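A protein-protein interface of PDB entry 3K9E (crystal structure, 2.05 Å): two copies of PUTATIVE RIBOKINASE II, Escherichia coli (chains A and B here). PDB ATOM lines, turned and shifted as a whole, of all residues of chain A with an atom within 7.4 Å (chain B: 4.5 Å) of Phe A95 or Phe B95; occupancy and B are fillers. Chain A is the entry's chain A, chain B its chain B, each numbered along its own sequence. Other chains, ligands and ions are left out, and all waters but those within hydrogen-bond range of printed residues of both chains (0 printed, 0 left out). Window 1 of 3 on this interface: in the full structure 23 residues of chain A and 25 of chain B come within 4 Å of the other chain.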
ATOM      1  N   LEU A  13      -0.076  19.826 -16.400  1.00  0.00           N
ATOM      2  CA  LEU A  13       0.070  18.573 -15.680  1.00  0.00           C
ATOM      3  C   LEU A  13      -0.872  17.506 -16.202  1.00  0.00           C
ATOM      4  O   LEU A  13      -1.687  17.762 -17.083  1.00  0.00           O
ATOM      5  CB  LEU A  13      -0.199  18.795 -14.190  1.00  0.00           C
ATOM      6  CG  LEU A  13      -1.526  19.460 -13.798  1.00  0.00           C
ATOM      7  CD1 LEU A  13      -2.124  18.756 -12.596  1.00  0.00           C
ATOM      8  CD2 LEU A  13      -1.289  20.923 -13.488  1.00  0.00           C
ATOM      9  N   VAL A  14      -0.742  16.298 -15.672  1.00  0.00           N
ATOM     10  CA  VAL A  14      -1.631  15.216 -16.075  1.00  0.00           C
ATOM     11  C   VAL A  14      -2.502  14.870 -14.877  1.00  0.00           C
ATOM     12  O   VAL A  14      -2.066  14.976 -13.721  1.00  0.00           O
ATOM     13  CB  VAL A  14      -0.867  13.934 -16.509  1.00  0.00           C
ATOM     14  CG1 VAL A  14       0.020  14.231 -17.721  1.00  0.00           C
ATOM     15  CG2 VAL A  14      -0.049  13.378 -15.336  1.00  0.00           C
ATOM     16  N   GLU A  15      -3.738  14.476 -15.147  1.00  0.00           N
ATOM     17  CA  GLU A  15      -4.628  14.099 -14.072  1.00  0.00           C
ATOM     18  C   GLU A  15      -4.904  12.602 -14.154  1.00  0.00           C
ATOM     19  O   GLU A  15      -5.108  12.068 -15.237  1.00  0.00           O
ATOM     20  CB  GLU A  15      -5.943  14.874 -14.159  1.00  0.00           C
ATOM     21  CG  GLU A  15      -6.702  14.849 -12.846  1.00  0.00           C
ATOM     22  CD  GLU A  15      -8.004  15.621 -12.891  1.00  0.00           C
ATOM     23  OE1 GLU A  15      -8.974  15.107 -13.484  1.00  0.00           O
ATOM     24  OE2 GLU A  15      -8.052  16.737 -12.334  1.00  0.00           O
ATOM     25  N   ILE A  16      -4.885  11.942 -13.002  1.00  0.00           N
ATOM     26  CA  ILE A  16      -5.149  10.509 -12.890  1.00  0.00           C
ATOM     27  C   ILE A  16      -6.464  10.436 -12.100  1.00  0.00           C
ATOM     28  O   ILE A  16      -6.540  10.937 -10.973  1.00  0.00           O
ATOM     29  CB  ILE A  16      -4.032   9.810 -12.082  1.00  0.00           C
ATOM     30  CG1 ILE A  16      -2.663  10.116 -12.708  1.00  0.00           C
ATOM     31  CG2 ILE A  16      -4.298   8.311 -12.017  1.00  0.00           C
ATOM     32  CD1 ILE A  16      -2.387   9.384 -14.018  1.00  0.00           C
ATOM     33  N   MET A  17      -7.491   9.817 -12.677  1.00  0.00           N
ATOM     34  CA  MET A  17      -8.800   9.757 -12.023  1.00  0.00           C
ATOM     35  C   MET A  17      -9.245   8.414 -11.462  1.00  0.00           C
ATOM     36  O   MET A  17      -9.149   7.391 -12.131  1.00  0.00           O
ATOM     37  CB  MET A  17      -9.870  10.243 -13.001  1.00  0.00           C
ATOM     38  CG  MET A  17      -9.628  11.642 -13.549  1.00  0.00           C
ATOM     39  SD  MET A  17     -11.020  12.158 -14.796  1.00  0.00           S
ATOM     40  CE  MET A  17     -12.433  12.502 -13.516  1.00  0.00           C
ATOM     41  N   ALA A  18      -9.767   8.429 -10.239  1.00  0.00           N
ATOM     42  CA  ALA A  18     -10.257   7.207  -9.610  1.00  0.00           C
ATOM     43  C   ALA A  18     -11.342   6.631 -10.514  1.00  0.00           C
ATOM     44  O   ALA A  18     -12.095   7.376 -11.144  1.00  0.00           O
ATOM     45  CB  ALA A  18     -10.831   7.515  -8.221  1.00  0.00           C
ATOM     46  N   PHE A  25      -7.439   6.823  -1.552  1.00  0.00           N
ATOM     47  CA  PHE A  25      -6.074   6.994  -2.033  1.00  0.00           C
ATOM     48  C   PHE A  25      -5.143   5.981  -1.357  1.00  0.00           C
ATOM     49  O   PHE A  25      -4.049   5.712  -1.854  1.00  0.00           O
ATOM     50  CB  PHE A  25      -5.553   8.400  -1.710  1.00  0.00           C
ATOM     51  CG  PHE A  25      -6.071   9.481  -2.621  1.00  0.00           C
ATOM     52  CD1 PHE A  25      -5.994   9.347  -3.999  1.00  0.00           C
ATOM     53  CD2 PHE A  25      -6.580  10.664  -2.091  1.00  0.00           C
ATOM     54  CE1 PHE A  25      -6.413  10.374  -4.844  1.00  0.00           C
ATOM     55  CE2 PHE A  25      -7.002  11.702  -2.931  1.00  0.00           C
ATOM     56  CZ  PHE A  25      -6.917  11.554  -4.310  1.00  0.00           C
ATOM     57  N   TRP A  31      -7.267   3.038 -11.722  1.00  0.00           N
ATOM     58  CA  TRP A  31      -7.239   4.454 -12.076  1.00  0.00           C
ATOM     59  C   TRP A  31      -7.235   4.647 -13.578  1.00  0.00           C
ATOM     60  O   TRP A  31      -6.719   3.807 -14.324  1.00  0.00           O
ATOM     61  CB  TRP A  31      -6.001   5.141 -11.489  1.00  0.00           C
ATOM     62  CG  TRP A  31      -5.941   5.088  -9.992  1.00  0.00           C
ATOM     63  CD1 TRP A  31      -5.606   4.013  -9.222  1.00  0.00           C
ATOM     64  CD2 TRP A  31      -6.316   6.129  -9.085  1.00  0.00           C
ATOM     65  NE1 TRP A  31      -5.752   4.319  -7.887  1.00  0.00           N
ATOM     66  CE2 TRP A  31      -6.185   5.618  -7.778  1.00  0.00           C
ATOM     67  CE3 TRP A  31      -6.748   7.452  -9.252  1.00  0.00           C
ATOM     68  CZ2 TRP A  31      -6.482   6.374  -6.645  1.00  0.00           C
ATOM     69  CZ3 TRP A  31      -7.044   8.207  -8.122  1.00  0.00           C
ATOM     70  CH2 TRP A  31      -6.905   7.667  -6.837  1.00  0.00           C
ATOM     71  N   GLY A  33      -6.268   7.292 -16.792  1.00  0.00           N
ATOM     72  CA  GLY A  33      -5.399   8.408 -17.112  1.00  0.00           C
ATOM     73  C   GLY A  33      -4.131   7.967 -17.819  1.00  0.00           C
ATOM     74  O   GLY A  33      -3.989   6.794 -18.170  1.00  0.00           O
ATOM     75  N   PRO A  34      -3.186   8.889 -18.046  1.00  0.00           N
ATOM     76  CA  PRO A  34      -3.272  10.305 -17.666  1.00  0.00           C
ATOM     77  C   PRO A  34      -4.144  11.123 -18.623  1.00  0.00           C
ATOM     78  O   PRO A  34      -4.326  10.730 -19.765  1.00  0.00           O
ATOM     79  CB  PRO A  34      -1.815  10.754 -17.727  1.00  0.00           C
ATOM     80  CG  PRO A  34      -1.314   9.991 -18.916  1.00  0.00           C
ATOM     81  CD  PRO A  34      -1.886   8.598 -18.678  1.00  0.00           C
ATOM     82  N   PHE A  65       4.191  11.940 -19.634  1.00  0.00           N
ATOM     83  CA  PHE A  65       3.176  12.826 -19.085  1.00  0.00           C
ATOM     84  C   PHE A  65       3.362  14.211 -19.673  1.00  0.00           C
ATOM     85  O   PHE A  65       2.394  14.926 -19.902  1.00  0.00           O
ATOM     86  CB  PHE A  65       3.270  12.861 -17.558  1.00  0.00           C
ATOM     87  CG  PHE A  65       2.817  11.583 -16.905  1.00  0.00           C
ATOM     88  CD1 PHE A  65       2.252  10.563 -17.670  1.00  0.00           C
ATOM     89  CD2 PHE A  65       2.939  11.402 -15.530  1.00  0.00           C
ATOM     90  CE1 PHE A  65       1.814   9.383 -17.078  1.00  0.00           C
ATOM     91  CE2 PHE A  65       2.499  10.219 -14.922  1.00  0.00           C
ATOM     92  CZ  PHE A  65       1.937   9.211 -15.693  1.00  0.00           C
ATOM     93  N   SER A  93       1.595  16.245 -11.712  1.00  0.00           N
ATOM     94  CA  SER A  93       0.455  15.338 -11.778  1.00  0.00           C
ATOM     95  C   SER A  93      -0.532  15.604 -10.647  1.00  0.00           C
ATOM     96  O   SER A  93      -0.227  16.311  -9.689  1.00  0.00           O
ATOM     97  CB  SER A  93       0.932  13.889 -11.693  1.00  0.00           C
ATOM     98  OG  SER A  93       1.528  13.657 -10.427  1.00  0.00           O
ATOM     99  N   ALA A  94      -1.715  15.016 -10.764  1.00  0.00           N
ATOM    100  CA  ALA A  94      -2.756  15.169  -9.765  1.00  0.00           C
ATOM    101  C   ALA A  94      -3.676  13.962  -9.788  1.00  0.00           C
ATOM    102  O   ALA A  94      -4.226  13.616 -10.834  1.00  0.00           O
ATOM    103  CB  ALA A  94      -3.572  16.436 -10.030  1.00  0.00           C
ATOM    104  N   PHE A  95      -3.817  13.313  -8.639  1.00  0.00           N
ATOM    105  CA  PHE A  95      -4.710  12.165  -8.499  1.00  0.00           C
ATOM    106  C   PHE A  95      -5.986  12.723  -7.887  1.00  0.00           C
ATOM    107  O   PHE A  95      -5.932  13.515  -6.944  1.00  0.00           O
ATOM    108  CB  PHE A  95      -4.119  11.121  -7.548  1.00  0.00           C
ATOM    109  CG  PHE A  95      -2.930  10.399  -8.102  1.00  0.00           C
ATOM    110  CD1 PHE A  95      -3.056   9.116  -8.622  1.00  0.00           C
ATOM    111  CD2 PHE A  95      -1.684  11.006  -8.114  1.00  0.00           C
ATOM    112  CE1 PHE A  95      -1.949   8.448  -9.148  1.00  0.00           C
ATOM    113  CE2 PHE A  95      -0.576  10.352  -8.635  1.00  0.00           C
ATOM    114  CZ  PHE A  95      -0.710   9.070  -9.154  1.00  0.00           C
ATOM    115  N   VAL A  96      -7.132  12.320  -8.420  1.00  0.00           N
ATOM    116  CA  VAL A  96      -8.393  12.811  -7.894  1.00  0.00           C
ATOM    117  C   VAL A  96      -9.403  11.699  -7.688  1.00  0.00           C
ATOM    118  O   VAL A  96      -9.424  10.717  -8.429  1.00  0.00           O
ATOM    119  CB  VAL A  96      -9.013  13.878  -8.829  1.00  0.00           C
ATOM    120  CG1 VAL A  96      -9.177  13.311 -10.232  1.00  0.00           C
ATOM    121  CG2 VAL A  96     -10.361  14.321  -8.290  1.00  0.00           C
ATOM    122  N   THR A  97     -10.221  11.857  -6.654  1.00  0.00           N
ATOM    123  CA  THR A  97     -11.273  10.905  -6.345  1.00  0.00           C
ATOM    124  C   THR A  97     -12.512  11.698  -5.940  1.00  0.00           C
ATOM    125  O   THR A  97     -12.404  12.817  -5.443  1.00  0.00           O
ATOM    126  CB  THR A  97     -10.874   9.957  -5.205  1.00  0.00           C
ATOM    127  OG1 THR A  97     -11.971   9.077  -4.927  1.00  0.00           O
ATOM    128  CG2 THR A  97     -10.514  10.737  -3.950  1.00  0.00           C
ATOM    129  N   ASP A 105     -11.422  15.231  -3.859  1.00  0.00           N
ATOM    130  CA  ASP A 105     -10.143  15.127  -3.150  1.00  0.00           C
ATOM    131  C   ASP A 105      -8.976  14.863  -4.102  1.00  0.00           C
ATOM    132  O   ASP A 105      -9.118  14.122  -5.073  1.00  0.00           O
ATOM    133  CB  ASP A 105     -10.207  14.017  -2.106  1.00  0.00           C
ATOM    134  CG  ASP A 105     -10.288  14.555  -0.697  1.00  0.00           C
ATOM    135  OD1 ASP A 105     -11.279  15.255  -0.374  1.00  0.00           O
ATOM    136  OD2 ASP A 105      -9.351  14.278   0.087  1.00  0.00           O
ATOM    137  N   PHE A 106      -7.820  15.450  -3.801  1.00  0.00           N
ATOM    138  CA  PHE A 106      -6.639  15.312  -4.654  1.00  0.00           C
ATOM    139  C   PHE A 106      -5.326  15.050  -3.932  1.00  0.00           C
ATOM    140  O   PHE A 106      -5.189  15.286  -2.731  1.00  0.00           O
ATOM    141  CB  PHE A 106      -6.379  16.603  -5.438  1.00  0.00           C
ATOM    142  CG  PHE A 106      -7.535  17.098  -6.246  1.00  0.00           C
ATOM    143  CD1 PHE A 106      -7.526  16.978  -7.631  1.00  0.00           C
ATOM    144  CD2 PHE A 106      -8.585  17.777  -5.637  1.00  0.00           C
ATOM    145  CE1 PHE A 106      -8.546  17.531  -8.398  1.00  0.00           C
ATOM    146  CE2 PHE A 106      -9.611  18.334  -6.398  1.00  0.00           C
ATOM    147  CZ  PHE A 106      -9.589  18.217  -7.776  1.00  0.00           C
ATOM    148  N   ILE A 107      -4.356  14.577  -4.706  1.00  0.00           N
ATOM    149  CA  ILE A 107      -2.985  14.404  -4.239  1.00  0.00           C
ATOM    150  C   ILE A 107      -2.250  15.107  -5.373  1.00  0.00           C
ATOM    151  O   ILE A 107      -2.254  14.644  -6.520  1.00  0.00           O
ATOM    152  CB  ILE A 107      -2.517  12.939  -4.140  1.00  0.00           C
ATOM    153  CG1 ILE A 107      -3.198  12.255  -2.944  1.00  0.00           C
ATOM    154  CG2 ILE A 107      -0.986  12.907  -3.963  1.00  0.00           C
ATOM    155  CD1 ILE A 107      -2.519  10.961  -2.492  1.00  0.00           C
ATOM    156  N   PHE A 108      -1.674  16.257  -5.056  1.00  0.00           N
ATOM    157  CA  PHE A 108      -0.978  17.077  -6.039  1.00  0.00           C
ATOM    158  C   PHE A 108       0.531  17.013  -6.016  1.00  0.00           C
ATOM    159  O   PHE A 108       1.141  16.989  -4.950  1.00  0.00           O
ATOM    160  CB  PHE A 108      -1.309  18.564  -5.838  1.00  0.00           C
ATOM    161  CG  PHE A 108      -2.717  18.943  -6.157  1.00  0.00           C
ATOM    162  CD1 PHE A 108      -3.218  18.797  -7.443  1.00  0.00           C
ATOM    163  CD2 PHE A 108      -3.529  19.506  -5.173  1.00  0.00           C
ATOM    164  CE1 PHE A 108      -4.505  19.210  -7.752  1.00  0.00           C
ATOM    165  CE2 PHE A 108      -4.823  19.923  -5.470  1.00  0.00           C
ATOM    166  CZ  PHE A 108      -5.313  19.777  -6.761  1.00  0.00           C
ATOM    167  N   ASN A 109       1.122  17.008  -7.204  1.00  0.00           N
ATOM    168  CA  ASN A 109       2.567  17.109  -7.347  1.00  0.00           C
ATOM    169  C   ASN A 109       2.749  18.177  -8.420  1.00  0.00           C
ATOM    170  O   ASN A 109       2.884  17.862  -9.600  1.00  0.00           O
ATOM    171  CB  ASN A 109       3.251  15.828  -7.819  1.00  0.00           C
ATOM    172  CG  ASN A 109       4.773  16.002  -7.860  1.00  0.00           C
ATOM    173  OD1 ASN A 109       5.344  16.628  -6.961  1.00  0.00           O
ATOM    174  ND2 ASN A 109       5.423  15.475  -8.889  1.00  0.00           N
ATOM    175  N   ILE B  16       2.408   2.750  -9.203  1.00  0.00           N
ATOM    176  CA  ILE B  16       1.178   2.708  -9.995  1.00  0.00           C
ATOM    177  C   ILE B  16       1.597   1.935 -11.239  1.00  0.00           C
ATOM    178  O   ILE B  16       2.473   2.374 -11.986  1.00  0.00           O
ATOM    179  CB  ILE B  16       0.709   4.124 -10.394  1.00  0.00           C
ATOM    180  CG1 ILE B  16       0.234   4.881  -9.154  1.00  0.00           C
ATOM    181  CG2 ILE B  16      -0.405   4.040 -11.414  1.00  0.00           C
ATOM    182  CD1 ILE B  16       1.338   5.229  -8.199  1.00  0.00           C
ATOM    183  N   PHE B  25       2.911   5.739 -21.730  1.00  0.00           N
ATOM    184  CA  PHE B  25       2.743   6.765 -20.705  1.00  0.00           C
ATOM    185  C   PHE B  25       1.992   7.977 -21.270  1.00  0.00           C
ATOM    186  O   PHE B  25       1.334   8.711 -20.531  1.00  0.00           O
ATOM    187  CB  PHE B  25       4.109   7.265 -20.206  1.00  0.00           C
ATOM    188  CG  PHE B  25       4.798   6.343 -19.235  1.00  0.00           C
ATOM    189  CD1 PHE B  25       4.144   5.895 -18.092  1.00  0.00           C
ATOM    190  CD2 PHE B  25       6.119   5.964 -19.442  1.00  0.00           C
ATOM    191  CE1 PHE B  25       4.796   5.083 -17.169  1.00  0.00           C
ATOM    192  CE2 PHE B  25       6.786   5.149 -18.523  1.00  0.00           C
ATOM    193  CZ  PHE B  25       6.123   4.710 -17.387  1.00  0.00           C
ATOM    194  N   TRP B  31      -4.714   1.999 -14.979  1.00  0.00           N
ATOM    195  CA  TRP B  31      -3.567   1.753 -14.110  1.00  0.00           C
ATOM    196  C   TRP B  31      -4.014   1.133 -12.797  1.00  0.00           C
ATOM    197  O   TRP B  31      -5.140   1.356 -12.357  1.00  0.00           O
ATOM    198  CB  TRP B  31      -2.817   3.066 -13.831  1.00  0.00           C
ATOM    199  CG  TRP B  31      -2.328   3.766 -15.079  1.00  0.00           C
ATOM    200  CD1 TRP B  31      -3.066   4.543 -15.929  1.00  0.00           C
ATOM    201  CD2 TRP B  31      -1.002   3.727 -15.625  1.00  0.00           C
ATOM    202  NE1 TRP B  31      -2.279   4.995 -16.966  1.00  0.00           N
ATOM    203  CE2 TRP B  31      -1.005   4.513 -16.800  1.00  0.00           C
ATOM    204  CE3 TRP B  31       0.197   3.113 -15.224  1.00  0.00           C
ATOM    205  CZ2 TRP B  31       0.136   4.692 -17.594  1.00  0.00           C
ATOM    206  CZ3 TRP B  31       1.336   3.290 -16.011  1.00  0.00           C
ATOM    207  CH2 TRP B  31       1.295   4.082 -17.183  1.00  0.00           C
ATOM    208  N   PHE B  65      -1.157   8.218  -0.059  1.00  0.00           N
ATOM    209  CA  PHE B  65      -0.085   7.382  -0.585  1.00  0.00           C
ATOM    210  C   PHE B  65       0.913   7.113   0.536  1.00  0.00           C
ATOM    211  O   PHE B  65       1.480   6.019   0.642  1.00  0.00           O
ATOM    212  CB  PHE B  65       0.613   8.088  -1.750  1.00  0.00           C
ATOM    213  CG  PHE B  65      -0.216   8.163  -3.003  1.00  0.00           C
ATOM    214  CD1 PHE B  65      -1.379   7.405  -3.140  1.00  0.00           C
ATOM    215  CD2 PHE B  65       0.188   8.963  -4.065  1.00  0.00           C
ATOM    216  CE1 PHE B  65      -2.127   7.448  -4.319  1.00  0.00           C
ATOM    217  CE2 PHE B  65      -0.548   9.012  -5.246  1.00  0.00           C
ATOM    218  CZ  PHE B  65      -1.703   8.259  -5.377  1.00  0.00           C
ATOM    219  N   ALA B  94       6.037   6.149  -8.415  1.00  0.00           N
ATOM    220  CA  ALA B  94       6.678   5.604  -9.602  1.00  0.00           C
ATOM    221  C   ALA B  94       5.616   4.936 -10.477  1.00  0.00           C
ATOM    222  O   ALA B  94       4.836   4.117 -10.003  1.00  0.00           O
ATOM    223  CB  ALA B  94       7.754   4.588  -9.201  1.00  0.00           C
ATOM    224  N   PHE B  95       5.573   5.325 -11.743  1.00  0.00           N
ATOM    225  CA  PHE B  95       4.646   4.739 -12.704  1.00  0.00           C
ATOM    226  C   PHE B  95       5.493   3.754 -13.490  1.00  0.00           C
ATOM    227  O   PHE B  95       6.614   4.075 -13.881  1.00  0.00           O
ATOM    228  CB  PHE B  95       4.104   5.801 -13.664  1.00  0.00           C
ATOM    229  CG  PHE B  95       3.015   6.643 -13.087  1.00  0.00           C
ATOM    230  CD1 PHE B  95       1.680   6.279 -13.249  1.00  0.00           C
ATOM    231  CD2 PHE B  95       3.316   7.801 -12.377  1.00  0.00           C
ATOM    232  CE1 PHE B  95       0.661   7.050 -12.717  1.00  0.00           C
ATOM    233  CE2 PHE B  95       2.299   8.587 -11.836  1.00  0.00           C
ATOM    234  CZ  PHE B  95       0.965   8.206 -12.009  1.00  0.00           C
ATOM    235  N   VAL B  96       4.976   2.558 -13.721  1.00  0.00           N
ATOM    236  CA  VAL B  96       5.749   1.582 -14.475  1.00  0.00           C
ATOM    237  C   VAL B  96       4.930   0.867 -15.550  1.00  0.00           C
ATOM    238  O   VAL B  96       3.752   0.568 -15.361  1.00  0.00           O
ATOM    239  CB  VAL B  96       6.380   0.511 -13.533  1.00  0.00           C
ATOM    240  CG1 VAL B  96       5.290  -0.231 -12.779  1.00  0.00           C
ATOM    241  CG2 VAL B  96       7.214  -0.468 -14.342  1.00  0.00           C
ATOM    242  N   THR B  97       5.564   0.636 -16.697  1.00  0.00           N
ATOM    243  CA  THR B  97       4.929  -0.096 -17.780  1.00  0.00           C
ATOM    244  C   THR B  97       5.834  -1.228 -18.197  1.00  0.00           C
ATOM    245  O   THR B  97       7.032  -1.218 -17.912  1.00  0.00           O
ATOM    246  CB  THR B  97       4.693   0.716 -19.054  1.00  0.00           C
ATOM    247  OG1 THR B  97       4.388   2.078 -18.738  1.00  0.00           O
ATOM    248  CG2 THR B  97       3.526   0.091 -19.813  1.00  0.00           C
ATOM    249  N   ASP B 105       9.638   0.434 -17.956  1.00  0.00           N
ATOM    250  CA  ASP B 105       9.830   1.863 -18.164  1.00  0.00           C
ATOM    251  C   ASP B 105       9.233   2.517 -16.937  1.00  0.00           C
ATOM    252  O   ASP B 105       8.174   2.104 -16.480  1.00  0.00           O
ATOM    253  CB  ASP B 105       9.086   2.322 -19.418  1.00  0.00           C
ATOM    254  CG  ASP B 105      10.018   2.589 -20.571  1.00  0.00           C
ATOM    255  OD1 ASP B 105      10.887   1.730 -20.812  1.00  0.00           O
ATOM    256  OD2 ASP B 105       9.894   3.636 -21.249  1.00  0.00           O
ATOM    257  N   PHE B 106       9.887   3.544 -16.405  1.00  0.00           N
ATOM    258  CA  PHE B 106       9.392   4.208 -15.199  1.00  0.00           C
ATOM    259  C   PHE B 106       9.358   5.723 -15.339  1.00  0.00           C
ATOM    260  O   PHE B 106      10.127   6.310 -16.087  1.00  0.00           O
ATOM    261  CB  PHE B 106      10.320   3.925 -14.022  1.00  0.00           C
ATOM    262  CG  PHE B 106      10.418   2.478 -13.631  1.00  0.00           C
ATOM    263  CD1 PHE B 106       9.667   1.987 -12.579  1.00  0.00           C
ATOM    264  CD2 PHE B 106      11.315   1.624 -14.262  1.00  0.00           C
ATOM    265  CE1 PHE B 106       9.816   0.670 -12.137  1.00  0.00           C
ATOM    266  CE2 PHE B 106      11.477   0.298 -13.834  1.00  0.00           C
ATOM    267  CZ  PHE B 106      10.723  -0.185 -12.766  1.00  0.00           C
ATOM    268  N   ILE B 107       8.456   6.344 -14.589  1.00  0.00           N
ATOM    269  CA  ILE B 107       8.345   7.801 -14.492  1.00  0.00           C
ATOM    270  C   ILE B 107       8.455   7.927 -12.989  1.00  0.00           C
ATOM    271  O   ILE B 107       7.499   7.635 -12.269  1.00  0.00           O
ATOM    272  CB  ILE B 107       6.977   8.353 -14.967  1.00  0.00           C
ATOM    273  CG1 ILE B 107       6.922   8.326 -16.503  1.00  0.00           C
ATOM    274  CG2 ILE B 107       6.741   9.762 -14.388  1.00  0.00           C
ATOM    275  CD1 ILE B 107       5.814   9.184 -17.096  1.00  0.00           C
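The backbone carbonyl oxygen (O) of Trp A31 sits at hydrogen-bond distance from the backbone NH (N) of Trp B31 (2.8 Å).
The indole nitrogen of Trp B31 is in hydrogen-bond range of the backbone carbonyl oxygen of Gly A33 (2.8 Å).
Phe A25 touches Phe B65, and with the chains exchanged Phe A65 touches Phe B25.
Trp A31 touches its own counterpart, Trp B31.
Phe A65 touches Phe B95, and with the chains exchanged Phe A95 touches Phe B65.
Phe B95 touches its own counterpart, Phe A95.
Of the 11 printed residues of chain B, 5 touch a printed residue of chain A.
Of the 21 printed residues of chain A, 7 touch a printed residue of chain B.
Printed residues of chain A that touch a printed residue of chain B: Phe A25, Trp A31, Gly A33, Pro A34, Phe A65, Phe A95 and Ile A107.
Hydrophobic or aromatic side chains of chain A within 4 Å of the printed part of chain B: Trp A31, Pro A34, Phe A65, Phe A95 and Ile A107.
Among the printed residues, no Asp or Glu carboxylate lies within 4 Å of a Lys or Arg side-chain nitrogen of the other chain.
Phe A25 touches Phe B65 (O to CD1, 3.4 Å).
Phe B25 touches Pro A34 (O to CG, 3.4 Å).
Phe A65 touches Phe B25 (CD1 to O, 3.5 Å).
CE2 of Phe A65 touches CE2 of Phe B95, 3.5 Å away.
CG of Phe A65 touches CD1 of Ile B107, at 3.8 Å.
Phe B65 touches Phe A95 (CZ to CD1, 3.6 Å).
Phe B95 touches Phe A95 (CZ to CZ, 3.4 Å).
Ile A107 touches Phe B65.
The backbone carbonyl oxygen of Phe A95 sits at hydrogen-bond distance from the backbone NH of Ile A107 (2.9 Å).
The backbone carbonyl oxygen (O) of Phe B95 is in hydrogen-bond range of the backbone NH (N) of Ile B107 (3.0 Å).
Printed residues of chain B within 4 Å of Phe A65: Phe B25, Phe B95 and Ile B107.
Phe A95 touches just these residues of chain B: Phe B65 and Phe B95.
Phe A106 touches none of the printed residues of chain B.
Of the printed residues of chain A, Phe B65 touches Phe A25 (3.4 Å), Phe A95 (3.6 Å) and Ile A107 (3.7 Å).
The nearest residue of chain B that does not touch Phe A95 is Ile B16 (4.2 Å).
The nearest printed residue of chain B that does not touch Gly A33 is Phe B25 (6.1 Å).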
